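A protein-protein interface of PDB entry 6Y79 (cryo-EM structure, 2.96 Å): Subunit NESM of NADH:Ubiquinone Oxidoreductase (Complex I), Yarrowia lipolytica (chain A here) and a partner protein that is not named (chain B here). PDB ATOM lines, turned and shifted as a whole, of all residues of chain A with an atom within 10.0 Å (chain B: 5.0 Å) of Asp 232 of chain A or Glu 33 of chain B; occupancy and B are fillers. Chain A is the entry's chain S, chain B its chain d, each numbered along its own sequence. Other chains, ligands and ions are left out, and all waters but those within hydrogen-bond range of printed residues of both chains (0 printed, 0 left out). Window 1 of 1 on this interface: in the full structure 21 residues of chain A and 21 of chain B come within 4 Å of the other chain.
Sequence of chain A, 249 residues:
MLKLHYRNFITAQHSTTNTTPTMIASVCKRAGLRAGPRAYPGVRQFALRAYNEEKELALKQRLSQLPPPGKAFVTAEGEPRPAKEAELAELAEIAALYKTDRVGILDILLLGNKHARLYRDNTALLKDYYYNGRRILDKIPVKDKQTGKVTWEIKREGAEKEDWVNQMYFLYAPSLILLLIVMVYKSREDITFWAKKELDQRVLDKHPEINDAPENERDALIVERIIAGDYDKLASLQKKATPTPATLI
Of the 11 printed residues of chain B, 7 touch a printed residue of chain A. Of the 21 printed residues of chain A, 12 touch a printed residue of chain B. Hydrophobic or aromatic side chains of chain A that line the printed part of chain B: Ile 191, Trp 194, Ala 195, Leu 199, Leu 234 and Leu 237. Among the printed residues, Asp or Glu carboxylates within 4 Å of a Lys or Arg side-chain nitrogen of the other chain: Arg 202 of chain A with Glu 33 of chain B (2.6 Å) and Asp 232 of chain A with Arg 37 of chain B (3.6 Å).
OD2 of Asp 232 of chain A lies within salt-bridge range of NE of Arg 37 of chain B (3.6 Å). O of Asp 232 of chain A sits close to OE1 of Glu 33 of chain B, at 2.7 Å. NH2 of Arg 202 of chain A lies within salt-bridge range of OE2 of Glu 33 of chain B (2.6 Å). The side-chain amide nitrogen of Gln 238 of chain A sits at hydrogen-bond distance from the side-chain hydroxyl of Tyr 30 of chain B, 3.3 Å away.
CG of Arg 32 of chain B touches CD1 of Ile 191 of chain A, at 3.8 Å. CG1 of Ile 191 of chain A touches CD2 of Phe 35 of chain B, at 3.6 Å. Arg 32 of chain B touches Trp 194 of chain A. Ala 195 of chain A touches Ile 36 of chain B. Glu 198 of chain A touches Ile 36 of chain B. Leu 9 of chain B touches Lys 233 of chain A. Tyr 30 of chain B touches Leu 234 of chain A. CD2 of Leu 234 of chain A touches NH2 of Arg 37 of chain B, 3.4 Å away. CD1 of Leu 237 of chain A touches CA of Tyr 30 of chain B, at 3.9 Å. Glu 33 of chain B touches Leu 237 of chain A (CG to CD1, 3.8 Å).
Asp 232 of chain A touches just these residues of chain B: Glu 33 and Arg 37. Of the printed residues of chain A, Glu 33 of chain B touches Arg 202, Asp 232 and Leu 237. Arg 37 of chain B touches just these residues of chain A: Asp 232 (3.2 Å) and Leu 234 (3.4 Å). Of the printed residues of chain A, Arg 32 of chain B touches Ile 191 (3.8 Å) and Trp 194 (3.5 Å). Printed residues of chain B within 4 Å of Ala 195 of chain A: Ile 36. Of the printed residues of chain B, Leu 234 of chain A touches Tyr 30 (3.8 Å) and Arg 37 (3.4 Å). Of the printed residues of chain B, Trp 194 of chain A touches Arg 32. Val 203 of chain A touches none of the printed residues of chain B. Ser 236 of chain A touches none of the printed residues of chain B. The nearest residue of chain B that does not touch Asp 232 of chain A is Ile 36 of chain B (4.3 Å). The nearest residue of chain A that does not touch Glu 33 of chain B is Leu 234 of chain A (4.3 Å). The nearest printed residue of chain B that does not touch Gln 238 of chain A is Arg 37 of chain B (6.7 Å).
NH1 of Arg 202 of chain A is in hydrogen-bond range of O of Asp 232 of chain A, at 2.5 Å. The backbone carbonyl oxygen (O) of Tyr 231 of chain A sits at hydrogen-bond distance from the guanidinium group (NH1) of Arg 202 of chain A, at 3.2 Å. The backbone carbonyl oxygen (O) of Glu 28 of chain B is in hydrogen-bond range of the guanidinium group (NE) of Arg 32 of chain B (3.3 Å). The side-chain carboxylate (OE2) of Glu 198 of chain A lies within salt-bridge range of the guanidinium group (NE) of Arg 202 of chain A, at 3.3 Å.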
ATOM      1  N   ILE A 191     -17.647  12.731 -29.386  1.00  0.00           N
ATOM      2  CA  ILE A 191     -17.322  12.765 -27.970  1.00  0.00           C
ATOM      3  C   ILE A 191     -15.835  13.011 -27.739  1.00  0.00           C
ATOM      4  O   ILE A 191     -15.429  13.406 -26.644  1.00  0.00           O
ATOM      5  CB  ILE A 191     -17.815  11.451 -27.333  1.00  0.00           C
ATOM      6  CG1 ILE A 191     -17.919  11.556 -25.811  1.00  0.00           C
ATOM      7  CG2 ILE A 191     -16.963  10.291 -27.800  1.00  0.00           C
ATOM      8  CD1 ILE A 191     -19.100  12.346 -25.341  1.00  0.00           C
ATOM      9  N   TRP A 194     -15.353  16.960 -28.146  1.00  0.00           N
ATOM     10  CA  TRP A 194     -16.055  17.504 -26.991  1.00  0.00           C
ATOM     11  C   TRP A 194     -15.356  17.152 -25.688  1.00  0.00           C
ATOM     12  O   TRP A 194     -15.316  17.974 -24.769  1.00  0.00           O
ATOM     13  CB  TRP A 194     -17.501  17.000 -26.970  1.00  0.00           C
ATOM     14  CG  TRP A 194     -18.266  17.476 -25.781  1.00  0.00           C
ATOM     15  CD1 TRP A 194     -18.981  18.631 -25.673  1.00  0.00           C
ATOM     16  CD2 TRP A 194     -18.378  16.817 -24.519  1.00  0.00           C
ATOM     17  NE1 TRP A 194     -19.530  18.729 -24.423  1.00  0.00           N
ATOM     18  CE2 TRP A 194     -19.169  17.629 -23.694  1.00  0.00           C
ATOM     19  CE3 TRP A 194     -17.873  15.623 -24.006  1.00  0.00           C
ATOM     20  CZ2 TRP A 194     -19.473  17.281 -22.391  1.00  0.00           C
ATOM     21  CZ3 TRP A 194     -18.171  15.284 -22.719  1.00  0.00           C
ATOM     22  CH2 TRP A 194     -18.965  16.106 -21.923  1.00  0.00           C
ATOM     23  N   ALA A 195     -14.774  15.960 -25.596  1.00  0.00           N
ATOM     24  CA  ALA A 195     -14.128  15.540 -24.362  1.00  0.00           C
ATOM     25  C   ALA A 195     -12.784  16.216 -24.165  1.00  0.00           C
ATOM     26  O   ALA A 195     -12.414  16.513 -23.022  1.00  0.00           O
ATOM     27  CB  ALA A 195     -13.965  14.024 -24.339  1.00  0.00           C
ATOM     28  N   GLU A 198     -13.776  19.596 -22.967  1.00  0.00           N
ATOM     29  CA  GLU A 198     -14.253  19.545 -21.591  1.00  0.00           C
ATOM     30  C   GLU A 198     -13.105  19.396 -20.602  1.00  0.00           C
ATOM     31  O   GLU A 198     -13.120  20.020 -19.537  1.00  0.00           O
ATOM     32  CB  GLU A 198     -15.256  18.405 -21.427  1.00  0.00           C
ATOM     33  CG  GLU A 198     -15.796  18.231 -20.012  1.00  0.00           C
ATOM     34  CD  GLU A 198     -16.719  19.356 -19.601  1.00  0.00           C
ATOM     35  OE1 GLU A 198     -17.379  19.927 -20.490  1.00  0.00           O
ATOM     36  OE2 GLU A 198     -16.787  19.669 -18.395  1.00  0.00           O
ATOM     37  N   LEU A 199     -12.096  18.588 -20.937  1.00  0.00           N
ATOM     38  CA  LEU A 199     -10.947  18.419 -20.050  1.00  0.00           C
ATOM     39  C   LEU A 199     -10.127  19.705 -19.948  1.00  0.00           C
ATOM     40  O   LEU A 199      -9.673  20.079 -18.851  1.00  0.00           O
ATOM     41  CB  LEU A 199     -10.094  17.259 -20.554  1.00  0.00           C
ATOM     42  CG  LEU A 199      -8.908  16.740 -19.752  1.00  0.00           C
ATOM     43  CD1 LEU A 199      -9.335  16.318 -18.372  1.00  0.00           C
ATOM     44  CD2 LEU A 199      -8.293  15.572 -20.486  1.00  0.00           C
ATOM     45  N   ARG A 202     -12.064  22.013 -17.747  1.00  0.00           N
ATOM     46  CA  ARG A 202     -11.966  21.657 -16.334  1.00  0.00           C
ATOM     47  C   ARG A 202     -10.650  22.117 -15.720  1.00  0.00           C
ATOM     48  O   ARG A 202     -10.619  22.554 -14.559  1.00  0.00           O
ATOM     49  CB  ARG A 202     -12.138  20.153 -16.159  1.00  0.00           C
ATOM     50  CG  ARG A 202     -13.562  19.695 -16.309  1.00  0.00           C
ATOM     51  CD  ARG A 202     -13.684  18.217 -16.053  1.00  0.00           C
ATOM     52  NE  ARG A 202     -15.014  17.724 -16.381  1.00  0.00           N
ATOM     53  CZ  ARG A 202     -15.395  16.463 -16.226  1.00  0.00           C
ATOM     54  NH1 ARG A 202     -14.547  15.569 -15.744  1.00  0.00           N
ATOM     55  NH2 ARG A 202     -16.625  16.095 -16.550  1.00  0.00           N
ATOM     56  N   VAL A 203      -9.547  22.029 -16.465  1.00  0.00           N
ATOM     57  CA  VAL A 203      -8.303  22.506 -15.861  1.00  0.00           C
ATOM     58  C   VAL A 203      -8.232  24.031 -15.896  1.00  0.00           C
ATOM     59  O   VAL A 203      -7.564  24.645 -15.057  1.00  0.00           O
ATOM     60  CB  VAL A 203      -7.072  21.849 -16.503  1.00  0.00           C
ATOM     61  CG1 VAL A 203      -7.102  20.363 -16.248  1.00  0.00           C
ATOM     62  CG2 VAL A 203      -7.005  22.133 -17.973  1.00  0.00           C
ATOM     63  N   LYS A 206     -10.196  24.865 -12.632  1.00  0.00           N
ATOM     64  CA  LYS A 206      -9.519  24.753 -11.343  1.00  0.00           C
ATOM     65  C   LYS A 206      -8.368  25.746 -11.222  1.00  0.00           C
ATOM     66  O   LYS A 206      -8.178  26.354 -10.163  1.00  0.00           O
ATOM     67  CB  LYS A 206      -9.019  23.326 -11.127  1.00  0.00           C
ATOM     68  CG  LYS A 206      -8.471  23.089  -9.734  1.00  0.00           C
ATOM     69  CD  LYS A 206      -8.071  21.646  -9.538  1.00  0.00           C
ATOM     70  CE  LYS A 206      -9.294  20.752  -9.440  1.00  0.00           C
ATOM     71  NZ  LYS A 206     -10.054  20.968  -8.179  1.00  0.00           N
ATOM     72  N   ARG A 225      -0.725  20.294 -16.388  1.00  0.00           N
ATOM     73  CA  ARG A 225      -1.777  20.114 -15.396  1.00  0.00           C
ATOM     74  C   ARG A 225      -2.550  18.815 -15.600  1.00  0.00           C
ATOM     75  O   ARG A 225      -2.965  18.194 -14.616  1.00  0.00           O
ATOM     76  CB  ARG A 225      -2.730  21.307 -15.408  1.00  0.00           C
ATOM     77  CG  ARG A 225      -2.108  22.575 -14.866  1.00  0.00           C
ATOM     78  CD  ARG A 225      -1.568  22.385 -13.462  1.00  0.00           C
ATOM     79  NE  ARG A 225      -0.989  23.622 -12.953  1.00  0.00           N
ATOM     80  CZ  ARG A 225      -0.384  23.739 -11.776  1.00  0.00           C
ATOM     81  NH1 ARG A 225      -0.282  22.686 -10.977  1.00  0.00           N
ATOM     82  NH2 ARG A 225       0.115  24.908 -11.397  1.00  0.00           N
ATOM     83  N   ILE A 226      -2.737  18.388 -16.855  1.00  0.00           N
ATOM     84  CA  ILE A 226      -3.415  17.119 -17.131  1.00  0.00           C
ATOM     85  C   ILE A 226      -2.572  15.948 -16.642  1.00  0.00           C
ATOM     86  O   ILE A 226      -3.091  14.967 -16.096  1.00  0.00           O
ATOM     87  CB  ILE A 226      -3.740  16.997 -18.633  1.00  0.00           C
ATOM     88  CG1 ILE A 226      -4.761  18.038 -19.059  1.00  0.00           C
ATOM     89  CG2 ILE A 226      -4.330  15.646 -18.973  1.00  0.00           C
ATOM     90  CD1 ILE A 226      -4.826  18.215 -20.552  1.00  0.00           C
ATOM     91  N   ALA A 228      -0.438  16.224 -14.165  1.00  0.00           N
ATOM     92  CA  ALA A 228      -0.317  16.348 -12.720  1.00  0.00           C
ATOM     93  C   ALA A 228      -1.565  15.926 -11.951  1.00  0.00           C
ATOM     94  O   ALA A 228      -1.495  15.823 -10.723  1.00  0.00           O
ATOM     95  CB  ALA A 228       0.034  17.789 -12.346  1.00  0.00           C
ATOM     96  N   GLY A 229      -2.694  15.674 -12.611  1.00  0.00           N
ATOM     97  CA  GLY A 229      -3.925  15.449 -11.877  1.00  0.00           C
ATOM     98  C   GLY A 229      -4.926  14.609 -12.631  1.00  0.00           C
ATOM     99  O   GLY A 229      -4.902  14.538 -13.863  1.00  0.00           O
ATOM    100  N   ASP A 230      -5.839  13.989 -11.872  1.00  0.00           N
ATOM    101  CA  ASP A 230      -6.877  13.132 -12.436  1.00  0.00           C
ATOM    102  C   ASP A 230      -7.872  13.915 -13.284  1.00  0.00           C
ATOM    103  O   ASP A 230      -8.009  13.644 -14.480  1.00  0.00           O
ATOM    104  CB  ASP A 230      -7.632  12.420 -11.318  1.00  0.00           C
ATOM    105  CG  ASP A 230      -6.772  11.457 -10.547  1.00  0.00           C
ATOM    106  OD1 ASP A 230      -5.598  11.246 -10.918  1.00  0.00           O
ATOM    107  OD2 ASP A 230      -7.290  10.902  -9.561  1.00  0.00           O
ATOM    108  N   TYR A 231      -8.605  14.841 -12.655  1.00  0.00           N
ATOM    109  CA  TYR A 231      -9.632  15.692 -13.282  1.00  0.00           C
ATOM    110  C   TYR A 231     -10.791  14.905 -13.875  1.00  0.00           C
ATOM    111  O   TYR A 231     -11.488  15.389 -14.764  1.00  0.00           O
ATOM    112  CB  TYR A 231      -9.048  16.610 -14.353  1.00  0.00           C
ATOM    113  CG  TYR A 231      -8.148  17.650 -13.781  1.00  0.00           C
ATOM    114  CD1 TYR A 231      -8.674  18.793 -13.204  1.00  0.00           C
ATOM    115  CD2 TYR A 231      -6.772  17.483 -13.782  1.00  0.00           C
ATOM    116  CE1 TYR A 231      -7.859  19.745 -12.656  1.00  0.00           C
ATOM    117  CE2 TYR A 231      -5.948  18.428 -13.237  1.00  0.00           C
ATOM    118  CZ  TYR A 231      -6.494  19.559 -12.675  1.00  0.00           C
ATOM    119  OH  TYR A 231      -5.666  20.512 -12.126  1.00  0.00           O
ATOM    120  N   ASP A 232     -11.035  13.690 -13.396  1.00  0.00           N
ATOM    121  CA  ASP A 232     -12.194  12.945 -13.890  1.00  0.00           C
ATOM    122  C   ASP A 232     -13.461  13.356 -13.158  1.00  0.00           C
ATOM    123  O   ASP A 232     -14.270  14.110 -13.706  1.00  0.00           O
ATOM    124  CB  ASP A 232     -11.964  11.441 -13.747  1.00  0.00           C
ATOM    125  CG  ASP A 232     -10.894  10.952 -14.679  1.00  0.00           C
ATOM    126  OD1 ASP A 232     -10.321  11.797 -15.382  1.00  0.00           O
ATOM    127  OD2 ASP A 232     -10.670   9.743 -14.700  1.00  0.00           O
ATOM    128  N   LYS A 233     -13.506  13.031 -11.855  1.00  0.00           N
ATOM    129  CA  LYS A 233     -14.676  12.799 -10.984  1.00  0.00           C
ATOM    130  C   LYS A 233     -15.347  11.451 -11.231  1.00  0.00           C
ATOM    131  O   LYS A 233     -16.576  11.369 -11.165  1.00  0.00           O
ATOM    132  CB  LYS A 233     -15.769  13.879 -11.033  1.00  0.00           C
ATOM    133  CG  LYS A 233     -15.288  15.297 -10.824  1.00  0.00           C
ATOM    134  CD  LYS A 233     -16.382  16.236 -11.269  1.00  0.00           C
ATOM    135  CE  LYS A 233     -15.882  17.643 -11.498  1.00  0.00           C
ATOM    136  NZ  LYS A 233     -17.043  18.565 -11.642  1.00  0.00           N
ATOM    137  N   LEU A 234     -14.603  10.387 -11.558  1.00  0.00           N
ATOM    138  CA  LEU A 234     -15.219   9.064 -11.650  1.00  0.00           C
ATOM    139  C   LEU A 234     -15.426   8.441 -10.274  1.00  0.00           C
ATOM    140  O   LEU A 234     -16.465   7.823 -10.023  1.00  0.00           O
ATOM    141  CB  LEU A 234     -14.380   8.133 -12.525  1.00  0.00           C
ATOM    142  CG  LEU A 234     -15.072   6.822 -12.913  1.00  0.00           C
ATOM    143  CD1 LEU A 234     -16.473   7.058 -13.437  1.00  0.00           C
ATOM    144  CD2 LEU A 234     -14.272   6.092 -13.955  1.00  0.00           C
ATOM    145  N   ALA A 235     -14.451   8.574  -9.370  1.00  0.00           N
ATOM    146  CA  ALA A 235     -14.655   8.131  -7.991  1.00  0.00           C
ATOM    147  C   ALA A 235     -15.673   8.993  -7.259  1.00  0.00           C
ATOM    148  O   ALA A 235     -16.232   8.548  -6.243  1.00  0.00           O
ATOM    149  CB  ALA A 235     -13.331   8.137  -7.232  1.00  0.00           C
ATOM    150  N   SER A 236     -15.899  10.221  -7.747  1.00  0.00           N
ATOM    151  CA  SER A 236     -17.046  10.989  -7.291  1.00  0.00           C
ATOM    152  C   SER A 236     -18.366  10.271  -7.592  1.00  0.00           C
ATOM    153  O   SER A 236     -19.306  10.341  -6.794  1.00  0.00           O
ATOM    154  CB  SER A 236     -17.030  12.368  -7.917  1.00  0.00           C
ATOM    155  OG  SER A 236     -18.292  12.951  -7.895  1.00  0.00           O
ATOM    156  N   LEU A 237     -18.475   9.592  -8.735  1.00  0.00           N
ATOM    157  CA  LEU A 237     -19.744   8.962  -9.103  1.00  0.00           C
ATOM    158  C   LEU A 237     -19.978   7.679  -8.317  1.00  0.00           C
ATOM    159  O   LEU A 237     -21.121   7.343  -8.000  1.00  0.00           O
ATOM    160  CB  LEU A 237     -19.779   8.679 -10.599  1.00  0.00           C
ATOM    161  CG  LEU A 237     -19.666   9.900 -11.501  1.00  0.00           C
ATOM    162  CD1 LEU A 237     -19.680   9.454 -12.943  1.00  0.00           C
ATOM    163  CD2 LEU A 237     -20.771  10.898 -11.240  1.00  0.00           C
ATOM    164  N   GLN A 238     -18.919   6.943  -8.011  1.00  0.00           N
ATOM    165  CA  GLN A 238     -19.031   5.673  -7.300  1.00  0.00           C
ATOM    166  C   GLN A 238     -18.981   5.871  -5.789  1.00  0.00           C
ATOM    167  O   GLN A 238     -18.100   5.361  -5.102  1.00  0.00           O
ATOM    168  CB  GLN A 238     -17.930   4.737  -7.774  1.00  0.00           C
ATOM    169  CG  GLN A 238     -17.750   4.766  -9.277  1.00  0.00           C
ATOM    170  CD  GLN A 238     -16.821   3.687  -9.774  1.00  0.00           C
ATOM    171  OE1 GLN A 238     -16.114   3.052  -8.996  1.00  0.00           O
ATOM    172  NE2 GLN A 238     -16.829   3.460 -11.077  1.00  0.00           N
ATOM    173  N   LEU B   9     -23.683  16.226 -13.545  1.00  0.00           N
ATOM    174  CA  LEU B   9     -23.218  14.883 -13.233  1.00  0.00           C
ATOM    175  C   LEU B   9     -24.133  14.220 -12.213  1.00  0.00           C
ATOM    176  O   LEU B   9     -24.442  14.799 -11.166  1.00  0.00           O
ATOM    177  CB  LEU B   9     -21.773  14.906 -12.734  1.00  0.00           C
ATOM    178  CG  LEU B   9     -20.741  15.163 -13.831  1.00  0.00           C
ATOM    179  CD1 LEU B   9     -19.346  15.095 -13.263  1.00  0.00           C
ATOM    180  CD2 LEU B   9     -20.894  14.172 -14.970  1.00  0.00           C
ATOM    181  N   GLU B  28     -25.373   8.322 -19.067  1.00  0.00           N
ATOM    182  CA  GLU B  28     -24.573   9.199 -19.917  1.00  0.00           C
ATOM    183  C   GLU B  28     -23.456   9.894 -19.146  1.00  0.00           C
ATOM    184  O   GLU B  28     -22.401  10.180 -19.722  1.00  0.00           O
ATOM    185  CB  GLU B  28     -25.466  10.241 -20.581  1.00  0.00           C
ATOM    186  CG  GLU B  28     -26.519   9.678 -21.501  1.00  0.00           C
ATOM    187  CD  GLU B  28     -27.342  10.770 -22.155  1.00  0.00           C
ATOM    188  OE1 GLU B  28     -27.138  11.950 -21.805  1.00  0.00           O
ATOM    189  OE2 GLU B  28     -28.193  10.458 -23.012  1.00  0.00           O
ATOM    190  N   SER B  29     -23.660  10.156 -17.851  1.00  0.00           N
ATOM    191  CA  SER B  29     -22.636  10.791 -17.031  1.00  0.00           C
ATOM    192  C   SER B  29     -21.425   9.893 -16.891  1.00  0.00           C
ATOM    193  O   SER B  29     -20.295  10.314 -17.156  1.00  0.00           O
ATOM    194  CB  SER B  29     -23.204  11.119 -15.651  1.00  0.00           C
ATOM    195  OG  SER B  29     -24.300  12.006 -15.735  1.00  0.00           O
ATOM    196  N   TYR B  30     -21.656   8.645 -16.480  1.00  0.00           N
ATOM    197  CA  TYR B  30     -20.587   7.666 -16.310  1.00  0.00           C
ATOM    198  C   TYR B  30     -19.860   7.398 -17.628  1.00  0.00           C
ATOM    199  O   TYR B  30     -18.619   7.293 -17.661  1.00  0.00           O
ATOM    200  CB  TYR B  30     -21.221   6.403 -15.733  1.00  0.00           C
ATOM    201  CG  TYR B  30     -20.316   5.321 -15.236  1.00  0.00           C
ATOM    202  CD1 TYR B  30     -19.834   5.324 -13.940  1.00  0.00           C
ATOM    203  CD2 TYR B  30     -20.006   4.255 -16.044  1.00  0.00           C
ATOM    204  CE1 TYR B  30     -19.029   4.304 -13.486  1.00  0.00           C
ATOM    205  CE2 TYR B  30     -19.215   3.237 -15.604  1.00  0.00           C
ATOM    206  CZ  TYR B  30     -18.724   3.263 -14.327  1.00  0.00           C
ATOM    207  OH  TYR B  30     -17.924   2.232 -13.902  1.00  0.00           O
ATOM    208  N   THR B  31     -20.612   7.386 -18.734  1.00  0.00           N
ATOM    209  CA  THR B  31     -20.027   7.231 -20.066  1.00  0.00           C
ATOM    210  C   THR B  31     -19.088   8.387 -20.426  1.00  0.00           C
ATOM    211  O   THR B  31     -17.916   8.173 -20.786  1.00  0.00           O
ATOM    212  CB  THR B  31     -21.161   7.115 -21.082  1.00  0.00           C
ATOM    213  OG1 THR B  31     -21.837   5.868 -20.900  1.00  0.00           O
ATOM    214  CG2 THR B  31     -20.645   7.186 -22.474  1.00  0.00           C
ATOM    215  N   ARG B  32     -19.583   9.628 -20.322  1.00  0.00           N
ATOM    216  CA  ARG B  32     -18.777  10.792 -20.678  1.00  0.00           C
ATOM    217  C   ARG B  32     -17.581  10.967 -19.752  1.00  0.00           C
ATOM    218  O   ARG B  32     -16.538  11.477 -20.179  1.00  0.00           O
ATOM    219  CB  ARG B  32     -19.641  12.049 -20.672  1.00  0.00           C
ATOM    220  CG  ARG B  32     -20.608  12.131 -21.829  1.00  0.00           C
ATOM    221  CD  ARG B  32     -21.455  13.388 -21.774  1.00  0.00           C
ATOM    222  NE  ARG B  32     -22.392  13.366 -20.655  1.00  0.00           N
ATOM    223  CZ  ARG B  32     -22.304  14.164 -19.600  1.00  0.00           C
ATOM    224  NH1 ARG B  32     -23.194  14.080 -18.626  1.00  0.00           N
ATOM    225  NH2 ARG B  32     -21.326  15.052 -19.523  1.00  0.00           N
ATOM    226  N   GLU B  33     -17.687  10.505 -18.506  1.00  0.00           N
ATOM    227  CA  GLU B  33     -16.539  10.569 -17.612  1.00  0.00           C
ATOM    228  C   GLU B  33     -15.455   9.587 -18.024  1.00  0.00           C
ATOM    229  O   GLU B  33     -14.257   9.884 -17.891  1.00  0.00           O
ATOM    230  CB  GLU B  33     -16.969  10.317 -16.168  1.00  0.00           C
ATOM    231  CG  GLU B  33     -17.765  11.456 -15.546  1.00  0.00           C
ATOM    232  CD  GLU B  33     -17.095  12.788 -15.716  1.00  0.00           C
ATOM    233  OE1 GLU B  33     -15.879  12.854 -15.499  1.00  0.00           O
ATOM    234  OE2 GLU B  33     -17.767  13.770 -16.084  1.00  0.00           O
ATOM    235  N   GLN B  34     -15.854   8.420 -18.539  1.00  0.00           N
ATOM    236  CA  GLN B  34     -14.869   7.512 -19.124  1.00  0.00           C
ATOM    237  C   GLN B  34     -14.175   8.130 -20.335  1.00  0.00           C
ATOM    238  O   GLN B  34     -12.969   7.937 -20.533  1.00  0.00           O
ATOM    239  CB  GLN B  34     -15.537   6.205 -19.515  1.00  0.00           C
ATOM    240  CG  GLN B  34     -15.920   5.361 -18.351  1.00  0.00           C
ATOM    241  CD  GLN B  34     -16.612   4.115 -18.789  1.00  0.00           C
ATOM    242  OE1 GLN B  34     -16.916   3.947 -19.965  1.00  0.00           O
ATOM    243  NE2 GLN B  34     -16.869   3.225 -17.853  1.00  0.00           N
ATOM    244  N   PHE B  35     -14.910   8.900 -21.140  1.00  0.00           N
ATOM    245  CA  PHE B  35     -14.261   9.571 -22.272  1.00  0.00           C
ATOM    246  C   PHE B  35     -13.295  10.680 -21.834  1.00  0.00           C
ATOM    247  O   PHE B  35     -12.267  10.904 -22.496  1.00  0.00           O
ATOM    248  CB  PHE B  35     -15.307  10.123 -23.231  1.00  0.00           C
ATOM    249  CG  PHE B  35     -15.961   9.072 -24.071  1.00  0.00           C
ATOM    250  CD1 PHE B  35     -15.271   8.460 -25.102  1.00  0.00           C
ATOM    251  CD2 PHE B  35     -17.262   8.681 -23.827  1.00  0.00           C
ATOM    252  CE1 PHE B  35     -15.873   7.481 -25.867  1.00  0.00           C
ATOM    253  CE2 PHE B  35     -17.862   7.710 -24.594  1.00  0.00           C
ATOM    254  CZ  PHE B  35     -17.170   7.112 -25.610  1.00  0.00           C
ATOM    255  N   ILE B  36     -13.600  11.383 -20.738  1.00  0.00           N
ATOM    256  CA  ILE B  36     -12.676  12.389 -20.199  1.00  0.00           C
ATOM    257  C   ILE B  36     -11.380  11.730 -19.728  1.00  0.00           C
ATOM    258  O   ILE B  36     -10.266  12.200 -20.025  1.00  0.00           O
ATOM    259  CB  ILE B  36     -13.353  13.174 -19.059  1.00  0.00           C
ATOM    260  CG1 ILE B  36     -14.549  13.961 -19.578  1.00  0.00           C
ATOM    261  CG2 ILE B  36     -12.385  14.121 -18.395  1.00  0.00           C
ATOM    262  CD1 ILE B  36     -14.202  14.935 -20.642  1.00  0.00           C
ATOM    263  N   ARG B  37     -11.524  10.629 -18.979  1.00  0.00           N
ATOM    264  CA  ARG B  37     -10.415   9.754 -18.591  1.00  0.00           C
ATOM    265  C   ARG B  37      -9.559   9.337 -19.784  1.00  0.00           C
ATOM    266  O   ARG B  37      -8.313   9.348 -19.732  1.00  0.00           O
ATOM    267  CB  ARG B  37     -11.019   8.526 -17.922  1.00  0.00           C
ATOM    268  CG  ARG B  37     -10.105   7.718 -17.110  1.00  0.00           C
ATOM    269  CD  ARG B  37     -10.872   6.733 -16.279  1.00  0.00           C
ATOM    270  NE  ARG B  37     -10.031   6.218 -15.211  1.00  0.00           N
ATOM    271  CZ  ARG B  37     -10.303   5.132 -14.505  1.00  0.00           C
ATOM    272  NH1 ARG B  37      -9.483   4.738 -13.545  1.00  0.00           N
ATOM    273  NH2 ARG B  37     -11.386   4.428 -14.779  1.00  0.00           N
